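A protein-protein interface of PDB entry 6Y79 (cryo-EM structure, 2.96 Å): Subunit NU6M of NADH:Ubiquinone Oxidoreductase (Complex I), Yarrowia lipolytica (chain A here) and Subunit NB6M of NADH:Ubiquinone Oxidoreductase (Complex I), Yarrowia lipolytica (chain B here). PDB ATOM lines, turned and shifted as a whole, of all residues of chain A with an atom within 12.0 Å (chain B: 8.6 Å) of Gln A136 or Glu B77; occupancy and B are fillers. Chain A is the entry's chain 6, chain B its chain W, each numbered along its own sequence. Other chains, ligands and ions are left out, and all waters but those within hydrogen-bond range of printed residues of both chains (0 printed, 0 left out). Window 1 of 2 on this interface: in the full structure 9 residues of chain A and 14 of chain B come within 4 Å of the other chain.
Printed residues of chain B that touch a printed residue of chain A: Met B70, Leu B73, Gln B74 and Glu B77. Hydrophobic or aromatic side chains of chain B that line the printed part of chain A: Met B70 and Leu B73. Hydrophobic or aromatic side chains of chain A that line the printed part of chain B: Trp A138, Phe A139 and Ile A141. Along chain A the printed residues that touch a printed residue of chain B span positions 136 to 141.
OD1 of Asp B78 sits at hydrogen-bond distance from NE2 of Gln B74, 3.3 Å away. The side-chain hydroxyl of Thr B81 lies within hydrogen-bond range of the backbone carbonyl oxygen of Glu B77, 2.7 Å away.
No residue of chain B comes within 4 Å of Thr A135. Of the printed residues of chain B, Gln A136 touches Glu B77 (3.5 Å). Asp A137 touches none of the printed residues of chain B. Printed residues of chain B within 4 Å of Phe A139: Met B70 and Gln B74. Printed residues of chain B within 4 Å of Ile A141: Met B70. Of chain A, only Trp A138 (3.7 Å) comes within 4 Å of Leu B73. No residue of chain A comes within 4 Å of Ala B75. Glu B77 touches two residues of chain A. No residue of chain A comes within 4 Å of Arg B79. No residue of chain A comes within 4 Å of Gln B80. No residue of chain A comes within 4 Å of Thr B81. Arg B84 touches none of the printed residues of chain A. The nearest residue of chain B that does not touch Gln A136 is Gln B74 (5.7 Å). The nearest residue of chain A that does not touch Glu B77 is Asp A137 (5.4 Å). The nearest printed residue of chain A that does not touch Met B70 is Asn A140 (4.5 Å).
Among the printed residues, pairs that only touch across the chains: Trp A138 with Glu B77 (3.3 Å), Phe A139 with Gln B74 (3.4 Å), Phe A139 with Met B70 (3.4 Å), Gln A136 with Glu B77 (3.5 Å), Ile A141 with Met B70 (3.6 Å) and Trp A138 with Leu B73 (3.7 Å).
The side-chain amide oxygen of Gln B74 sits at hydrogen-bond distance from the backbone NH of Trp A138 (3.3 Å). The backbone carbonyl oxygen of Trp A138 lies close to the side-chain sulfur of Met B70 (3.6 Å).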
ATOM      1  N   THR A 132      36.176   3.535  11.194  1.00  0.00           N
ATOM      2  CA  THR A 132      35.305   3.255  10.058  1.00  0.00           C
ATOM      3  C   THR A 132      35.080   1.755   9.895  1.00  0.00           C
ATOM      4  O   THR A 132      35.980   0.945  10.112  1.00  0.00           O
ATOM      5  CB  THR A 132      35.873   3.892   8.772  1.00  0.00           C
ATOM      6  OG1 THR A 132      34.990   3.653   7.670  1.00  0.00           O
ATOM      7  CG2 THR A 132      37.272   3.412   8.436  1.00  0.00           C
ATOM      8  N   ILE A 133      33.839   1.385   9.612  1.00  0.00           N
ATOM      9  CA  ILE A 133      33.463  -0.012   9.444  1.00  0.00           C
ATOM     10  C   ILE A 133      33.578  -0.355   7.967  1.00  0.00           C
ATOM     11  O   ILE A 133      32.930   0.275   7.125  1.00  0.00           O
ATOM     12  CB  ILE A 133      32.044  -0.278   9.963  1.00  0.00           C
ATOM     13  CG1 ILE A 133      31.998  -0.136  11.481  1.00  0.00           C
ATOM     14  CG2 ILE A 133      31.577  -1.651   9.546  1.00  0.00           C
ATOM     15  CD1 ILE A 133      30.638  -0.393  12.078  1.00  0.00           C
ATOM     16  N   ILE A 134      34.402  -1.347   7.648  1.00  0.00           N
ATOM     17  CA  ILE A 134      34.605  -1.786   6.274  1.00  0.00           C
ATOM     18  C   ILE A 134      33.763  -3.033   6.039  1.00  0.00           C
ATOM     19  O   ILE A 134      33.903  -4.032   6.752  1.00  0.00           O
ATOM     20  CB  ILE A 134      36.087  -2.051   5.978  1.00  0.00           C
ATOM     21  CG1 ILE A 134      36.889  -0.756   6.074  1.00  0.00           C
ATOM     22  CG2 ILE A 134      36.246  -2.643   4.602  1.00  0.00           C
ATOM     23  CD1 ILE A 134      36.439   0.305   5.104  1.00  0.00           C
ATOM     24  N   THR A 135      32.890  -2.964   5.040  1.00  0.00           N
ATOM     25  CA  THR A 135      31.958  -4.016   4.669  1.00  0.00           C
ATOM     26  C   THR A 135      32.431  -4.634   3.358  1.00  0.00           C
ATOM     27  O   THR A 135      33.073  -3.964   2.545  1.00  0.00           O
ATOM     28  CB  THR A 135      30.538  -3.410   4.559  1.00  0.00           C
ATOM     29  OG1 THR A 135      30.052  -3.104   5.872  1.00  0.00           O
ATOM     30  CG2 THR A 135      29.496  -4.301   3.851  1.00  0.00           C
ATOM     31  N   GLN A 136      32.170  -5.925   3.167  1.00  0.00           N
ATOM     32  CA  GLN A 136      32.405  -6.558   1.880  1.00  0.00           C
ATOM     33  C   GLN A 136      31.122  -6.628   1.081  1.00  0.00           C
ATOM     34  O   GLN A 136      30.100  -7.117   1.568  1.00  0.00           O
ATOM     35  CB  GLN A 136      32.942  -7.956   2.066  1.00  0.00           C
ATOM     36  CG  GLN A 136      34.161  -7.918   2.839  1.00  0.00           C
ATOM     37  CD  GLN A 136      34.523  -9.286   3.272  1.00  0.00           C
ATOM     38  OE1 GLN A 136      33.900 -10.261   2.870  1.00  0.00           O
ATOM     39  NE2 GLN A 136      35.437  -9.380   4.220  1.00  0.00           N
ATOM     40  N   ASP A 137      31.177  -6.142  -0.141  1.00  0.00           N
ATOM     41  CA  ASP A 137      30.127  -6.376  -1.111  1.00  0.00           C
ATOM     42  C   ASP A 137      30.747  -7.034  -2.331  1.00  0.00           C
ATOM     43  O   ASP A 137      31.864  -6.694  -2.727  1.00  0.00           O
ATOM     44  CB  ASP A 137      29.427  -5.070  -1.467  1.00  0.00           C
ATOM     45  CG  ASP A 137      30.381  -4.035  -1.983  1.00  0.00           C
ATOM     46  OD1 ASP A 137      31.256  -3.599  -1.208  1.00  0.00           O
ATOM     47  OD2 ASP A 137      30.261  -3.653  -3.161  1.00  0.00           O
ATOM     48  N   TRP A 138      30.029  -7.993  -2.906  1.00  0.00           N
ATOM     49  CA  TRP A 138      30.532  -8.850  -3.976  1.00  0.00           C
ATOM     50  C   TRP A 138      30.084  -8.373  -5.347  1.00  0.00           C
ATOM     51  O   TRP A 138      29.748  -9.190  -6.197  1.00  0.00           O
ATOM     52  CB  TRP A 138      30.082 -10.292  -3.756  1.00  0.00           C
ATOM     53  CG  TRP A 138      30.620 -10.960  -2.528  1.00  0.00           C
ATOM     54  CD1 TRP A 138      30.068 -10.946  -1.292  1.00  0.00           C
ATOM     55  CD2 TRP A 138      31.796 -11.773  -2.433  1.00  0.00           C
ATOM     56  NE1 TRP A 138      30.833 -11.679  -0.424  1.00  0.00           N
ATOM     57  CE2 TRP A 138      31.900 -12.197  -1.101  1.00  0.00           C
ATOM     58  CE3 TRP A 138      32.778 -12.169  -3.343  1.00  0.00           C
ATOM     59  CZ2 TRP A 138      32.939 -12.998  -0.656  1.00  0.00           C
ATOM     60  CZ3 TRP A 138      33.805 -12.962  -2.901  1.00  0.00           C
ATOM     61  CH2 TRP A 138      33.874 -13.376  -1.572  1.00  0.00           C
ATOM     62  N   PHE A 139      30.032  -7.067  -5.592  1.00  0.00           N
ATOM     63  CA  PHE A 139      29.464  -6.556  -6.835  1.00  0.00           C
ATOM     64  C   PHE A 139      30.476  -6.390  -7.961  1.00  0.00           C
ATOM     65  O   PHE A 139      30.065  -6.139  -9.096  1.00  0.00           O
ATOM     66  CB  PHE A 139      28.787  -5.205  -6.604  1.00  0.00           C
ATOM     67  CG  PHE A 139      27.556  -5.270  -5.758  1.00  0.00           C
ATOM     68  CD1 PHE A 139      26.380  -5.800  -6.256  1.00  0.00           C
ATOM     69  CD2 PHE A 139      27.566  -4.760  -4.474  1.00  0.00           C
ATOM     70  CE1 PHE A 139      25.244  -5.839  -5.476  1.00  0.00           C
ATOM     71  CE2 PHE A 139      26.438  -4.795  -3.690  1.00  0.00           C
ATOM     72  CZ  PHE A 139      25.275  -5.331  -4.193  1.00  0.00           C
ATOM     73  N   ASN A 140      31.772  -6.513  -7.692  1.00  0.00           N
ATOM     74  CA  ASN A 140      32.812  -6.236  -8.678  1.00  0.00           C
ATOM     75  C   ASN A 140      33.517  -7.522  -9.079  1.00  0.00           C
ATOM     76  O   ASN A 140      34.065  -8.222  -8.227  1.00  0.00           O
ATOM     77  CB  ASN A 140      33.828  -5.240  -8.122  1.00  0.00           C
ATOM     78  CG  ASN A 140      34.818  -4.778  -9.164  1.00  0.00           C
ATOM     79  OD1 ASN A 140      34.578  -4.892 -10.365  1.00  0.00           O
ATOM     80  ND2 ASN A 140      35.950  -4.264  -8.708  1.00  0.00           N
ATOM     81  N   ILE A 141      33.554  -7.801 -10.380  1.00  0.00           N
ATOM     82  CA  ILE A 141      33.942  -9.110 -10.890  1.00  0.00           C
ATOM     83  C   ILE A 141      35.337  -9.142 -11.484  1.00  0.00           C
ATOM     84  O   ILE A 141      35.766 -10.211 -11.937  1.00  0.00           O
ATOM     85  CB  ILE A 141      32.923  -9.618 -11.924  1.00  0.00           C
ATOM     86  CG1 ILE A 141      32.622  -8.510 -12.925  1.00  0.00           C
ATOM     87  CG2 ILE A 141      31.678 -10.047 -11.245  1.00  0.00           C
ATOM     88  CD1 ILE A 141      31.595  -8.859 -13.948  1.00  0.00           C
ATOM     89  N   MET B  70      27.637 -14.354  -8.132  1.00  0.00           N
ATOM     90  CA  MET B  70      27.430 -13.113  -7.379  1.00  0.00           C
ATOM     91  C   MET B  70      26.175 -13.053  -6.497  1.00  0.00           C
ATOM     92  O   MET B  70      26.325 -12.695  -5.314  1.00  0.00           O
ATOM     93  CB  MET B  70      27.478 -11.907  -8.324  1.00  0.00           C
ATOM     94  CG  MET B  70      27.123 -10.613  -7.614  1.00  0.00           C
ATOM     95  SD  MET B  70      27.047  -9.152  -8.634  1.00  0.00           S
ATOM     96  CE  MET B  70      28.653  -9.230  -9.379  1.00  0.00           C
ATOM     97  N   PRO B  71      24.941 -13.355  -6.963  1.00  0.00           N
ATOM     98  CA  PRO B  71      23.783 -13.182  -6.059  1.00  0.00           C
ATOM     99  C   PRO B  71      23.782 -14.138  -4.885  1.00  0.00           C
ATOM    100  O   PRO B  71      23.256 -13.798  -3.818  1.00  0.00           O
ATOM    101  CB  PRO B  71      22.575 -13.436  -6.971  1.00  0.00           C
ATOM    102  CG  PRO B  71      23.080 -13.314  -8.328  1.00  0.00           C
ATOM    103  CD  PRO B  71      24.462 -13.832  -8.275  1.00  0.00           C
ATOM    104  N   LEU B  72      24.416 -15.296  -5.057  1.00  0.00           N
ATOM    105  CA  LEU B  72      24.538 -16.286  -3.999  1.00  0.00           C
ATOM    106  C   LEU B  72      25.342 -15.762  -2.817  1.00  0.00           C
ATOM    107  O   LEU B  72      24.999 -16.026  -1.660  1.00  0.00           O
ATOM    108  CB  LEU B  72      25.192 -17.534  -4.578  1.00  0.00           C
ATOM    109  CG  LEU B  72      25.418 -18.685  -3.625  1.00  0.00           C
ATOM    110  CD1 LEU B  72      24.077 -19.040  -3.037  1.00  0.00           C
ATOM    111  CD2 LEU B  72      26.015 -19.842  -4.384  1.00  0.00           C
ATOM    112  N   LEU B  73      26.418 -15.026  -3.083  1.00  0.00           N
ATOM    113  CA  LEU B  73      27.209 -14.446  -2.004  1.00  0.00           C
ATOM    114  C   LEU B  73      26.649 -13.106  -1.554  1.00  0.00           C
ATOM    115  O   LEU B  73      26.881 -12.680  -0.413  1.00  0.00           O
ATOM    116  CB  LEU B  73      28.653 -14.285  -2.461  1.00  0.00           C
ATOM    117  CG  LEU B  73      29.285 -15.563  -2.993  1.00  0.00           C
ATOM    118  CD1 LEU B  73      30.576 -15.253  -3.675  1.00  0.00           C
ATOM    119  CD2 LEU B  73      29.512 -16.519  -1.859  1.00  0.00           C
ATOM    120  N   GLN B  74      25.910 -12.431  -2.434  1.00  0.00           N
ATOM    121  CA  GLN B  74      25.317 -11.153  -2.073  1.00  0.00           C
ATOM    122  C   GLN B  74      24.185 -11.325  -1.072  1.00  0.00           C
ATOM    123  O   GLN B  74      24.055 -10.523  -0.140  1.00  0.00           O
ATOM    124  CB  GLN B  74      24.825 -10.433  -3.325  1.00  0.00           C
ATOM    125  CG  GLN B  74      24.449  -8.998  -3.074  1.00  0.00           C
ATOM    126  CD  GLN B  74      25.578  -8.223  -2.438  1.00  0.00           C
ATOM    127  OE1 GLN B  74      26.712  -8.269  -2.901  1.00  0.00           O
ATOM    128  NE2 GLN B  74      25.274  -7.503  -1.368  1.00  0.00           N
ATOM    129  N   ALA B  75      23.368 -12.372  -1.241  1.00  0.00           N
ATOM    130  CA  ALA B  75      22.353 -12.711  -0.250  1.00  0.00           C
ATOM    131  C   ALA B  75      22.978 -13.017   1.105  1.00  0.00           C
ATOM    132  O   ALA B  75      22.426 -12.633   2.149  1.00  0.00           O
ATOM    133  CB  ALA B  75      21.530 -13.893  -0.751  1.00  0.00           C
ATOM    134  N   GLU B  76      24.152 -13.661   1.090  1.00  0.00           N
ATOM    135  CA  GLU B  76      24.904 -13.951   2.311  1.00  0.00           C
ATOM    136  C   GLU B  76      25.291 -12.693   3.053  1.00  0.00           C
ATOM    137  O   GLU B  76      25.024 -12.544   4.257  1.00  0.00           O
ATOM    138  CB  GLU B  76      26.194 -14.693   1.988  1.00  0.00           C
ATOM    139  CG  GLU B  76      26.958 -14.975   3.199  1.00  0.00           C
ATOM    140  CD  GLU B  76      26.427 -16.165   3.913  1.00  0.00           C
ATOM    141  OE1 GLU B  76      25.848 -16.981   3.194  1.00  0.00           O
ATOM    142  OE2 GLU B  76      26.537 -16.241   5.150  1.00  0.00           O
ATOM    143  N   GLU B  77      26.002 -11.817   2.361  1.00  0.00           N
ATOM    144  CA  GLU B  77      26.500 -10.623   3.025  1.00  0.00           C
ATOM    145  C   GLU B  77      25.365  -9.671   3.375  1.00  0.00           C
ATOM    146  O   GLU B  77      25.471  -8.915   4.347  1.00  0.00           O
ATOM    147  CB  GLU B  77      27.560  -9.937   2.165  1.00  0.00           C
ATOM    148  CG  GLU B  77      28.835 -10.752   2.070  1.00  0.00           C
ATOM    149  CD  GLU B  77      29.594 -10.856   3.386  1.00  0.00           C
ATOM    150  OE1 GLU B  77      29.363 -11.814   4.159  1.00  0.00           O
ATOM    151  OE2 GLU B  77      30.434  -9.971   3.645  1.00  0.00           O
ATOM    152  N   ASP B  78      24.240  -9.765   2.663  1.00  0.00           N
ATOM    153  CA  ASP B  78      23.064  -8.984   3.025  1.00  0.00           C
ATOM    154  C   ASP B  78      22.460  -9.456   4.343  1.00  0.00           C
ATOM    155  O   ASP B  78      22.117  -8.636   5.203  1.00  0.00           O
ATOM    156  CB  ASP B  78      22.032  -9.050   1.904  1.00  0.00           C
ATOM    157  CG  ASP B  78      22.160  -7.895   0.934  1.00  0.00           C
ATOM    158  OD1 ASP B  78      23.130  -7.116   1.047  1.00  0.00           O
ATOM    159  OD2 ASP B  78      21.283  -7.761   0.060  1.00  0.00           O
ATOM    160  N   ARG B  79      22.334 -10.777   4.524  1.00  0.00           N
ATOM    161  CA  ARG B  79      21.822 -11.288   5.794  1.00  0.00           C
ATOM    162  C   ARG B  79      22.775 -11.005   6.945  1.00  0.00           C
ATOM    163  O   ARG B  79      22.320 -10.685   8.054  1.00  0.00           O
ATOM    164  CB  ARG B  79      21.545 -12.782   5.691  1.00  0.00           C
ATOM    165  CG  ARG B  79      20.279 -13.098   4.927  1.00  0.00           C
ATOM    166  CD  ARG B  79      20.120 -14.581   4.727  1.00  0.00           C
ATOM    167  NE  ARG B  79      21.134 -15.108   3.825  1.00  0.00           N
ATOM    168  CZ  ARG B  79      21.500 -16.381   3.784  1.00  0.00           C
ATOM    169  NH1 ARG B  79      20.938 -17.259   4.600  1.00  0.00           N
ATOM    170  NH2 ARG B  79      22.434 -16.777   2.934  1.00  0.00           N
ATOM    171  N   GLN B  80      24.088 -11.076   6.696  1.00  0.00           N
ATOM    172  CA  GLN B  80      25.049 -10.714   7.736  1.00  0.00           C
ATOM    173  C   GLN B  80      24.941  -9.240   8.105  1.00  0.00           C
ATOM    174  O   GLN B  80      24.991  -8.888   9.291  1.00  0.00           O
ATOM    175  CB  GLN B  80      26.472 -11.043   7.289  1.00  0.00           C
ATOM    176  CG  GLN B  80      26.777 -12.527   7.165  1.00  0.00           C
ATOM    177  CD  GLN B  80      26.554 -13.293   8.451  1.00  0.00           C
ATOM    178  OE1 GLN B  80      26.838 -12.804   9.543  1.00  0.00           O
ATOM    179  NE2 GLN B  80      26.038 -14.507   8.327  1.00  0.00           N
ATOM    180  N   THR B  81      24.738  -8.372   7.107  1.00  0.00           N
ATOM    181  CA  THR B  81      24.602  -6.940   7.355  1.00  0.00           C
ATOM    182  C   THR B  81      23.357  -6.635   8.180  1.00  0.00           C
ATOM    183  O   THR B  81      23.422  -5.874   9.158  1.00  0.00           O
ATOM    184  CB  THR B  81      24.567  -6.187   6.023  1.00  0.00           C
ATOM    185  OG1 THR B  81      25.786  -6.429   5.304  1.00  0.00           O
ATOM    186  CG2 THR B  81      24.420  -4.698   6.247  1.00  0.00           C
ATOM    187  N   VAL B  82      22.230  -7.268   7.824  1.00  0.00           N
ATOM    188  CA  VAL B  82      20.967  -7.059   8.534  1.00  0.00           C
ATOM    189  C   VAL B  82      21.092  -7.500   9.983  1.00  0.00           C
ATOM    190  O   VAL B  82      20.734  -6.756  10.906  1.00  0.00           O
ATOM    191  CB  VAL B  82      19.823  -7.803   7.827  1.00  0.00           C
ATOM    192  CG1 VAL B  82      18.591  -7.867   8.697  1.00  0.00           C
ATOM    193  CG2 VAL B  82      19.491  -7.120   6.529  1.00  0.00           C
ATOM    194  N   ARG B  83      21.654  -8.689  10.207  1.00  0.00           N
ATOM    195  CA  ARG B  83      21.778  -9.207  11.568  1.00  0.00           C
ATOM    196  C   ARG B  83      22.705  -8.367  12.443  1.00  0.00           C
ATOM    197  O   ARG B  83      22.306  -7.953  13.538  1.00  0.00           O
ATOM    198  CB  ARG B  83      22.259 -10.647  11.523  1.00  0.00           C
ATOM    199  CG  ARG B  83      22.388 -11.235  12.895  1.00  0.00           C
ATOM    200  CD  ARG B  83      22.995 -12.615  12.818  1.00  0.00           C
ATOM    201  NE  ARG B  83      24.341 -12.626  12.242  1.00  0.00           N
ATOM    202  CZ  ARG B  83      25.479 -12.497  12.926  1.00  0.00           C
ATOM    203  NH1 ARG B  83      26.625 -12.546  12.260  1.00  0.00           N
ATOM    204  NH2 ARG B  83      25.498 -12.335  14.249  1.00  0.00           N
ATOM    205  N   ARG B  84      23.898  -8.014  11.939  1.00  0.00           N
ATOM    206  CA  ARG B  84      24.844  -7.290  12.784  1.00  0.00           C
ATOM    207  C   ARG B  84      24.416  -5.849  13.023  1.00  0.00           C
ATOM    208  O   ARG B  84      24.693  -5.295  14.093  1.00  0.00           O
ATOM    209  CB  ARG B  84      26.229  -7.323  12.168  1.00  0.00           C
ATOM    210  CG  ARG B  84      26.759  -8.711  11.956  1.00  0.00           C
ATOM    211  CD  ARG B  84      28.053  -8.648  11.243  1.00  0.00           C
ATOM    212  NE  ARG B  84      28.961  -7.873  12.056  1.00  0.00           N
ATOM    213  CZ  ARG B  84      29.931  -8.408  12.772  1.00  0.00           C
ATOM    214  NH1 ARG B  84      30.713  -7.648  13.515  1.00  0.00           N
ATOM    215  NH2 ARG B  84      30.115  -9.712  12.734  1.00  0.00           N
ATOM    216  N   ALA B 115      23.492   0.588   6.793  1.00  0.00           N
ATOM    217  CA  ALA B 115      24.380  -0.052   7.743  1.00  0.00           C
ATOM    218  C   ALA B 115      25.122   1.012   8.546  1.00  0.00           C
ATOM    219  O   ALA B 115      25.519   2.042   7.994  1.00  0.00           O
ATOM    220  CB  ALA B 115      25.378  -0.953   7.023  1.00  0.00           C
